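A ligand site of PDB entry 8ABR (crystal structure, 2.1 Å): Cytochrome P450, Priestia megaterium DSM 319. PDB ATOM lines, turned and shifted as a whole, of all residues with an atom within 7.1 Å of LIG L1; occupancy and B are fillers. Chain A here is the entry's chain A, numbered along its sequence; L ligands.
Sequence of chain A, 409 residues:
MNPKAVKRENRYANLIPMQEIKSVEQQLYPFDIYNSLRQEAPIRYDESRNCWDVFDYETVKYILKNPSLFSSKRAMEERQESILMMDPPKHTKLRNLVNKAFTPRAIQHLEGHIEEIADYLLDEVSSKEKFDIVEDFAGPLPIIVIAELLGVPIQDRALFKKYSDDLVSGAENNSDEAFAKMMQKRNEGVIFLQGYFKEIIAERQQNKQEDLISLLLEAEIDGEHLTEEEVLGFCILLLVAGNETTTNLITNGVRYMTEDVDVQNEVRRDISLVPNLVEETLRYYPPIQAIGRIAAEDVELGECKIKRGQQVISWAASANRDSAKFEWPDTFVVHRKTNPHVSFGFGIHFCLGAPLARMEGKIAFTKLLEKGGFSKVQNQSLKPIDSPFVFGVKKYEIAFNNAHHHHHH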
ATOM      1  N   TYR A  12     -32.217  33.813  -7.906  1.00  0.00           N
ATOM      2  CA  TYR A  12     -31.177  32.936  -8.409  1.00  0.00           C
ATOM      3  C   TYR A  12     -30.331  33.669  -9.447  1.00  0.00           C
ATOM      4  O   TYR A  12     -30.839  34.058 -10.506  1.00  0.00           O
ATOM      5  CB  TYR A  12     -31.804  31.669  -9.000  1.00  0.00           C
ATOM      6  CG  TYR A  12     -30.831  30.532  -9.298  1.00  0.00           C
ATOM      7  CD1 TYR A  12     -29.678  30.351  -8.542  1.00  0.00           C
ATOM      8  CD2 TYR A  12     -31.092  29.640 -10.322  1.00  0.00           C
ATOM      9  CE1 TYR A  12     -28.812  29.304  -8.816  1.00  0.00           C
ATOM     10  CE2 TYR A  12     -30.239  28.588 -10.599  1.00  0.00           C
ATOM     11  CZ  TYR A  12     -29.087  28.431  -9.848  1.00  0.00           C
ATOM     12  OH  TYR A  12     -28.229  27.400 -10.125  1.00  0.00           O
ATOM     13  N   ASN A  14     -28.033  32.643 -11.417  1.00  0.00           N
ATOM     14  CA  ASN A  14     -27.725  31.904 -12.633  1.00  0.00           C
ATOM     15  C   ASN A  14     -28.757  32.156 -13.721  1.00  0.00           C
ATOM     16  O   ASN A  14     -28.529  31.758 -14.872  1.00  0.00           O
ATOM     17  CB  ASN A  14     -27.622  30.403 -12.328  1.00  0.00           C
ATOM     18  CG  ASN A  14     -26.618  29.692 -13.226  1.00  0.00           C
ATOM     19  OD1 ASN A  14     -25.632  30.291 -13.671  1.00  0.00           O
ATOM     20  ND2 ASN A  14     -26.855  28.389 -13.479  1.00  0.00           N
ATOM     21  N   LEU A  15     -29.883  32.791 -13.382  1.00  0.00           N
ATOM     22  CA  LEU A  15     -30.899  33.160 -14.346  1.00  0.00           C
ATOM     23  C   LEU A  15     -30.765  34.600 -14.831  1.00  0.00           C
ATOM     24  O   LEU A  15     -31.500  35.007 -15.740  1.00  0.00           O
ATOM     25  CB  LEU A  15     -32.299  32.984 -13.724  1.00  0.00           C
ATOM     26  CG  LEU A  15     -32.638  31.596 -13.155  1.00  0.00           C
ATOM     27  CD1 LEU A  15     -34.063  31.540 -12.640  1.00  0.00           C
ATOM     28  CD2 LEU A  15     -32.397  30.543 -14.235  1.00  0.00           C
ATOM     29  N   ARG A  74     -30.489  25.206  -4.030  1.00  0.00           N
ATOM     30  CA  ARG A  74     -30.577  26.546  -4.601  1.00  0.00           C
ATOM     31  C   ARG A  74     -31.926  26.789  -5.265  1.00  0.00           C
ATOM     32  O   ARG A  74     -32.051  27.707  -6.082  1.00  0.00           O
ATOM     33  CB  ARG A  74     -29.448  26.777  -5.607  1.00  0.00           C
ATOM     34  CG  ARG A  74     -29.483  25.822  -6.830  1.00  0.00           C
ATOM     35  CD  ARG A  74     -28.064  25.652  -7.354  1.00  0.00           C
ATOM     36  NE  ARG A  74     -27.944  24.948  -8.617  1.00  0.00           N
ATOM     37  CZ  ARG A  74     -27.704  23.644  -8.733  1.00  0.00           C
ATOM     38  NH1 ARG A  74     -27.761  22.836  -7.688  1.00  0.00           N
ATOM     39  NH2 ARG A  74     -27.384  23.147  -9.922  1.00  0.00           N
ATOM     40  N   LEU A  84     -31.102  17.121  -8.412  1.00  0.00           N
ATOM     41  CA  LEU A  84     -30.285  18.262  -8.803  1.00  0.00           C
ATOM     42  C   LEU A  84     -30.143  19.263  -7.667  1.00  0.00           C
ATOM     43  O   LEU A  84     -29.075  19.855  -7.484  1.00  0.00           O
ATOM     44  CB  LEU A  84     -30.894  18.960 -10.018  1.00  0.00           C
ATOM     45  CG  LEU A  84     -30.164  20.207 -10.525  1.00  0.00           C
ATOM     46  CD1 LEU A  84     -28.797  19.833 -11.044  1.00  0.00           C
ATOM     47  CD2 LEU A  84     -30.978  20.936 -11.614  1.00  0.00           C
ATOM     48  N   MET A  85     -31.207  19.431  -6.865  1.00  0.00           N
ATOM     49  CA  MET A  85     -31.264  20.443  -5.819  1.00  0.00           C
ATOM     50  C   MET A  85     -31.106  19.848  -4.435  1.00  0.00           C
ATOM     51  O   MET A  85     -31.459  20.506  -3.443  1.00  0.00           O
ATOM     52  CB  MET A  85     -32.574  21.221  -5.910  1.00  0.00           C
ATOM     53  CG  MET A  85     -32.860  21.837  -7.256  1.00  0.00           C
ATOM     54  SD  MET A  85     -32.086  23.441  -7.450  1.00  0.00           S
ATOM     55  CE  MET A  85     -32.166  23.669  -9.225  1.00  0.00           C
ATOM     56  N   LEU A 237     -37.133  16.731 -14.133  1.00  0.00           N
ATOM     57  CA  LEU A 237     -35.684  16.918 -14.310  1.00  0.00           C
ATOM     58  C   LEU A 237     -35.186  16.055 -15.450  1.00  0.00           C
ATOM     59  O   LEU A 237     -34.516  16.532 -16.373  1.00  0.00           O
ATOM     60  CB  LEU A 237     -34.936  16.593 -13.018  1.00  0.00           C
ATOM     61  CG  LEU A 237     -33.412  16.478 -13.087  1.00  0.00           C
ATOM     62  CD1 LEU A 237     -32.774  17.786 -13.553  1.00  0.00           C
ATOM     63  CD2 LEU A 237     -32.865  16.058 -11.721  1.00  0.00           C
ATOM     64  N   VAL A 240     -36.457  17.528 -18.890  1.00  0.00           N
ATOM     65  CA  VAL A 240     -35.846  18.778 -19.327  1.00  0.00           C
ATOM     66  C   VAL A 240     -34.365  18.581 -19.590  1.00  0.00           C
ATOM     67  O   VAL A 240     -33.857  19.004 -20.642  1.00  0.00           O
ATOM     68  CB  VAL A 240     -36.064  19.881 -18.273  1.00  0.00           C
ATOM     69  CG1 VAL A 240     -35.311  21.133 -18.675  1.00  0.00           C
ATOM     70  CG2 VAL A 240     -37.542  20.170 -18.080  1.00  0.00           C
ATOM     71  N   ALA A 241     -33.638  18.022 -18.610  1.00  0.00           N
ATOM     72  CA  ALA A 241     -32.214  17.766 -18.804  1.00  0.00           C
ATOM     73  C   ALA A 241     -31.984  16.858 -20.000  1.00  0.00           C
ATOM     74  O   ALA A 241     -31.072  17.075 -20.797  1.00  0.00           O
ATOM     75  CB  ALA A 241     -31.591  17.169 -17.536  1.00  0.00           C
ATOM     76  N   THR A 245     -30.511  20.165 -23.243  1.00  0.00           N
ATOM     77  CA  THR A 245     -29.065  20.190 -23.394  1.00  0.00           C
ATOM     78  C   THR A 245     -28.619  19.431 -24.629  1.00  0.00           C
ATOM     79  O   THR A 245     -27.775  19.913 -25.405  1.00  0.00           O
ATOM     80  CB  THR A 245     -28.451  19.582 -22.135  1.00  0.00           C
ATOM     81  OG1 THR A 245     -29.034  18.278 -21.958  1.00  0.00           O
ATOM     82  CG2 THR A 245     -28.718  20.417 -20.902  1.00  0.00           C
ATOM     83  N   ILE A 288     -24.451  23.822 -21.262  1.00  0.00           N
ATOM     84  CA  ILE A 288     -24.617  24.451 -19.952  1.00  0.00           C
ATOM     85  C   ILE A 288     -23.357  25.261 -19.681  1.00  0.00           C
ATOM     86  O   ILE A 288     -22.248  24.717 -19.660  1.00  0.00           O
ATOM     87  CB  ILE A 288     -24.860  23.420 -18.851  1.00  0.00           C
ATOM     88  CG1 ILE A 288     -26.172  22.651 -19.071  1.00  0.00           C
ATOM     89  CG2 ILE A 288     -24.864  24.105 -17.495  1.00  0.00           C
ATOM     90  CD1 ILE A 288     -27.421  23.478 -18.988  1.00  0.00           C
ATOM     91  N   ALA A 290     -22.948  27.619 -16.900  1.00  0.00           N
ATOM     92  CA  ALA A 290     -22.721  27.965 -15.501  1.00  0.00           C
ATOM     93  C   ALA A 290     -23.545  27.071 -14.603  1.00  0.00           C
ATOM     94  O   ALA A 290     -24.685  26.716 -14.924  1.00  0.00           O
ATOM     95  CB  ALA A 290     -23.065  29.442 -15.218  1.00  0.00           C
ATOM     96  N   ILE A 291     -22.965  26.712 -13.458  1.00  0.00           N
ATOM     97  CA  ILE A 291     -23.563  25.823 -12.482  1.00  0.00           C
ATOM     98  C   ILE A 291     -23.605  26.570 -11.154  1.00  0.00           C
ATOM     99  O   ILE A 291     -22.574  27.083 -10.683  1.00  0.00           O
ATOM    100  CB  ILE A 291     -22.776  24.511 -12.319  1.00  0.00           C
ATOM    101  CG1 ILE A 291     -22.627  23.772 -13.649  1.00  0.00           C
ATOM    102  CG2 ILE A 291     -23.448  23.614 -11.267  1.00  0.00           C
ATOM    103  CD1 ILE A 291     -21.582  22.618 -13.592  1.00  0.00           C
ATOM    104  N   GLY A 292     -24.767  26.583 -10.534  1.00  0.00           N
ATOM    105  CA  GLY A 292     -24.942  27.313  -9.293  1.00  0.00           C
ATOM    106  C   GLY A 292     -24.753  26.471  -8.059  1.00  0.00           C
ATOM    107  O   GLY A 292     -24.963  25.252  -8.047  1.00  0.00           O
ATOM    108  N   ARG A 293     -24.366  27.145  -6.978  1.00  0.00           N
ATOM    109  CA  ARG A 293     -24.172  26.542  -5.677  1.00  0.00           C
ATOM    110  C   ARG A 293     -24.456  27.626  -4.646  1.00  0.00           C
ATOM    111  O   ARG A 293     -24.431  28.822  -4.949  1.00  0.00           O
ATOM    112  CB  ARG A 293     -22.739  25.997  -5.506  1.00  0.00           C
ATOM    113  CG  ARG A 293     -22.409  24.752  -6.320  1.00  0.00           C
ATOM    114  CD  ARG A 293     -23.220  23.543  -5.845  1.00  0.00           C
ATOM    115  NE  ARG A 293     -22.730  22.295  -6.432  1.00  0.00           N
ATOM    116  CZ  ARG A 293     -23.201  21.756  -7.554  1.00  0.00           C
ATOM    117  NH1 ARG A 293     -24.139  22.364  -8.259  1.00  0.00           N
ATOM    118  NH2 ARG A 293     -22.720  20.596  -7.978  1.00  0.00           N
ATOM    119  N   ILE A 313     -21.542  31.075  -8.476  1.00  0.00           N
ATOM    120  CA  ILE A 313     -21.805  30.673  -9.851  1.00  0.00           C
ATOM    121  C   ILE A 313     -20.485  30.259 -10.475  1.00  0.00           C
ATOM    122  O   ILE A 313     -19.579  31.098 -10.625  1.00  0.00           O
ATOM    123  CB  ILE A 313     -22.448  31.814 -10.669  1.00  0.00           C
ATOM    124  CG1 ILE A 313     -23.682  32.365  -9.953  1.00  0.00           C
ATOM    125  CG2 ILE A 313     -22.772  31.338 -12.075  1.00  0.00           C
ATOM    126  CD1 ILE A 313     -24.763  31.346  -9.661  1.00  0.00           C
ATOM    127  N   CYS A 351     -23.315  14.688 -14.331  1.00  0.00           N
ATOM    128  CA  CYS A 351     -24.436  14.412 -15.200  1.00  0.00           C
ATOM    129  C   CYS A 351     -24.800  12.932 -15.289  1.00  0.00           C
ATOM    130  O   CYS A 351     -24.002  12.102 -15.713  1.00  0.00           O
ATOM    131  CB  CYS A 351     -24.126  14.915 -16.587  1.00  0.00           C
ATOM    132  SG  CYS A 351     -25.598  14.648 -17.654  1.00  0.00           S
ATOM    133  N   PHE A 389     -27.352  30.889 -18.457  1.00  0.00           N
ATOM    134  CA  PHE A 389     -26.613  29.670 -18.145  1.00  0.00           C
ATOM    135  C   PHE A 389     -26.686  28.626 -19.252  1.00  0.00           C
ATOM    136  O   PHE A 389     -26.090  27.544 -19.124  1.00  0.00           O
ATOM    137  CB  PHE A 389     -27.084  29.088 -16.798  1.00  0.00           C
ATOM    138  CG  PHE A 389     -28.374  28.286 -16.858  1.00  0.00           C
ATOM    139  CD1 PHE A 389     -28.349  26.924 -17.103  1.00  0.00           C
ATOM    140  CD2 PHE A 389     -29.589  28.892 -16.600  1.00  0.00           C
ATOM    141  CE1 PHE A 389     -29.489  26.173 -17.120  1.00  0.00           C
ATOM    142  CE2 PHE A 389     -30.753  28.133 -16.639  1.00  0.00           C
ATOM    143  CZ  PHE A 389     -30.690  26.751 -16.874  1.00  0.00           C
HETATM  144  C1  LIG L   1     -28.013  24.413 -14.021  1.00  0.00           C
HETATM  145  C2  LIG L   1     -27.808  25.331 -12.813  1.00  0.00           C
HETATM  146  O1  LIG L   1     -28.597  26.256 -12.651  1.00  0.00           O
HETATM  147  C3  LIG L   1     -27.133  23.168 -14.121  1.00  0.00           C
HETATM  148  C4  LIG L   1     -27.577  22.265 -15.264  1.00  0.00           C
HETATM  149  C5  LIG L   1     -28.329  21.021 -14.812  1.00  0.00           C
HETATM  150  C6  LIG L   1     -28.850  20.200 -15.992  1.00  0.00           C
HETATM  151  O2  LIG L   1     -26.835  25.060 -12.059  1.00  0.00           O
HETATM  152  C1  LG2 L   2     -37.885  23.782 -12.741  1.00  0.00           C
HETATM  153  C2  LG2 L   2     -37.318  22.413 -13.206  1.00  0.00           C
HETATM  154  C3  LG2 L   2     -35.842  22.142 -12.919  1.00  0.00           C
HETATM  155  C4  LG2 L   2     -35.247  21.095 -13.851  1.00  0.00           C
HETATM  156  C5  LG2 L   2     -34.370  21.667 -14.954  1.00  0.00           C
HETATM  157  C6  LG2 L   2     -32.921  21.950 -14.558  1.00  0.00           C
HETATM  158  C7  LG2 L   2     -32.076  22.586 -15.646  1.00  0.00           C
HETATM  159  C8  LG2 L   2     -31.954  21.769 -16.904  1.00  0.00           C
HETATM  160  O1  LG2 L   2     -38.850  23.806 -11.953  1.00  0.00           O
HETATM  161  O2  LG2 L   2     -37.302  24.790 -13.199  1.00  0.00           O
HETATM  162 FE1  LG3 L   3     -27.164  16.232 -17.378  1.00  0.00          FE
HETATM  163  C1  LG3 L   3     -26.713  16.854 -14.047  1.00  0.00           C
HETATM  164  C2  LG3 L   3     -25.243  18.918 -18.177  1.00  0.00           C
HETATM  165  C3  LG3 L   3     -27.649  15.606 -20.765  1.00  0.00           C
HETATM  166  C4  LG3 L   3     -29.772  14.128 -16.660  1.00  0.00           C
HETATM  167  N1  LG3 L   3     -26.211  17.637 -16.316  1.00  0.00           N
HETATM  168  C5  LG3 L   3     -26.026  17.670 -14.947  1.00  0.00           C
HETATM  169  C6  LG3 L   3     -25.019  18.688 -14.590  1.00  0.00           C
HETATM  170  C7  LG3 L   3     -24.620  19.222 -15.746  1.00  0.00           C
HETATM  171  C8  LG3 L   3     -25.380  18.591 -16.830  1.00  0.00           C
HETATM  172  C9  LG3 L   3     -23.596  20.367 -15.916  1.00  0.00           C
HETATM  173  C10 LG3 L   3     -24.483  19.018 -13.161  1.00  0.00           C
HETATM  174  C11 LG3 L   3     -25.202  20.159 -12.453  1.00  0.00           C
HETATM  175  C12 LG3 L   3     -24.729  20.330 -11.019  1.00  0.00           C
HETATM  176  O1  LG3 L   3     -23.562  20.014 -10.701  1.00  0.00           O
HETATM  177  O2  LG3 L   3     -25.543  20.799 -10.174  1.00  0.00           O
HETATM  178  N2  LG3 L   3     -26.611  17.134 -19.146  1.00  0.00           N
HETATM  179  C13 LG3 L   3     -25.753  18.198 -19.250  1.00  0.00           C
HETATM  180  C14 LG3 L   3     -25.396  18.391 -20.648  1.00  0.00           C
HETATM  181  C15 LG3 L   3     -26.049  17.472 -21.342  1.00  0.00           C
HETATM  182  C16 LG3 L   3     -26.785  16.640 -20.402  1.00  0.00           C
HETATM  183  C17 LG3 L   3     -24.440  19.474 -21.207  1.00  0.00           C
HETATM  184  C18 LG3 L   3     -26.068  17.200 -22.849  1.00  0.00           C
HETATM  185  C19 LG3 L   3     -25.009  17.436 -23.594  1.00  0.00           C
HETATM  186  N3  LG3 L   3     -28.487  15.191 -18.510  1.00  0.00           N
HETATM  187  C20 LG3 L   3     -28.408  14.898 -19.865  1.00  0.00           C
HETATM  188  C21 LG3 L   3     -29.292  13.795 -20.213  1.00  0.00           C
HETATM  189  C22 LG3 L   3     -29.876  13.396 -19.069  1.00  0.00           C
HETATM  190  C23 LG3 L   3     -29.372  14.233 -17.994  1.00  0.00           C
HETATM  191  C24 LG3 L   3     -29.456  13.218 -21.647  1.00  0.00           C
HETATM  192  C25 LG3 L   3     -30.873  12.238 -18.804  1.00  0.00           C
HETATM  193  C26 LG3 L   3     -31.161  11.357 -19.755  1.00  0.00           C
HETATM  194  N4  LG3 L   3     -28.052  15.599 -15.643  1.00  0.00           N
HETATM  195  C27 LG3 L   3     -29.149  14.774 -15.593  1.00  0.00           C
HETATM  196  C28 LG3 L   3     -29.535  14.678 -14.188  1.00  0.00           C
HETATM  197  C29 LG3 L   3     -28.704  15.436 -13.466  1.00  0.00           C
HETATM  198  C30 LG3 L   3     -27.766  16.029 -14.373  1.00  0.00           C
HETATM  199  C31 LG3 L   3     -30.752  13.863 -13.676  1.00  0.00           C
HETATM  200  C32 LG3 L   3     -28.733  15.609 -11.936  1.00  0.00           C
HETATM  201  C33 LG3 L   3     -27.706  14.634 -11.284  1.00  0.00           C
HETATM  202  C34 LG3 L   3     -27.542  14.899  -9.816  1.00  0.00           C
HETATM  203  O3  LG3 L   3     -26.999  14.019  -9.089  1.00  0.00           O
HETATM  204  O4  LG3 L   3     -27.946  15.990  -9.351  1.00  0.00           O
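An oxygen (O1) of LIG L1 sits at hydrogen-bond distance from the side-chain hydroxyl (OH) of Tyr 12. The side-chain amide nitrogen (ND2) of Asn 14 lies within hydrogen-bond range of an oxygen (O1) of LIG L1 (2.9 Å). NH2 of Arg 74 is in salt-bridge range of O2 of LIG L1, at 2.9 Å. N of Gly 292 lies within hydrogen-bond range of O2 of LIG L1 (3.0 Å). O2 of LG3 L3 is in salt-bridge range of NH2 of Arg 74, 3.0 Å away. O4 of LG3 L3 lies close to N of Leu 84 (3.5 Å). NH1 of Arg 293 lies within salt-bridge range of O2 of LG3 L3 (2.8 Å). SG of Cys 351 binds FE1 of LG3 L3 (2.2 Å).
NE of Arg 74 is in hydrogen-bond range of OH of Tyr 12 (2.9 Å). ND2 of Asn 14 is in hydrogen-bond range of O of Ala 290 (3.1 Å). The backbone carbonyl oxygen (O) of Gly 292 is in hydrogen-bond range of the guanidinium group (NE) of Arg 74 (3.1 Å). O of Leu 84 lies within hydrogen-bond range of NH1 of Arg 74.
Leu 84 touches LIG L1. Ile 288 touches LIG L1 (CD1 to C4, 3.9 Å). O of Ala 290 touches O2 of LIG L1 (3.9 Å). Ile 291 touches LIG L1 (CA to O2, 3.4 Å). Phe 389 touches LIG L1 (CE1 to C1, 3.9 Å). Hydrophobic or aromatic side chains within 4 Å of LIG L1: Tyr 12, Leu 84, Ile 288, Ile 291 and Phe 389. Nine residues have an atom within 4 Å of LIG L1: Tyr 12, Asn 14, Arg 74, Leu 84, Ile 288, Ala 290, Ile 291, Gly 292 and Phe 389. The nearest printed residue that does not touch LIG L1 is Ala 241 (4.4 Å).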
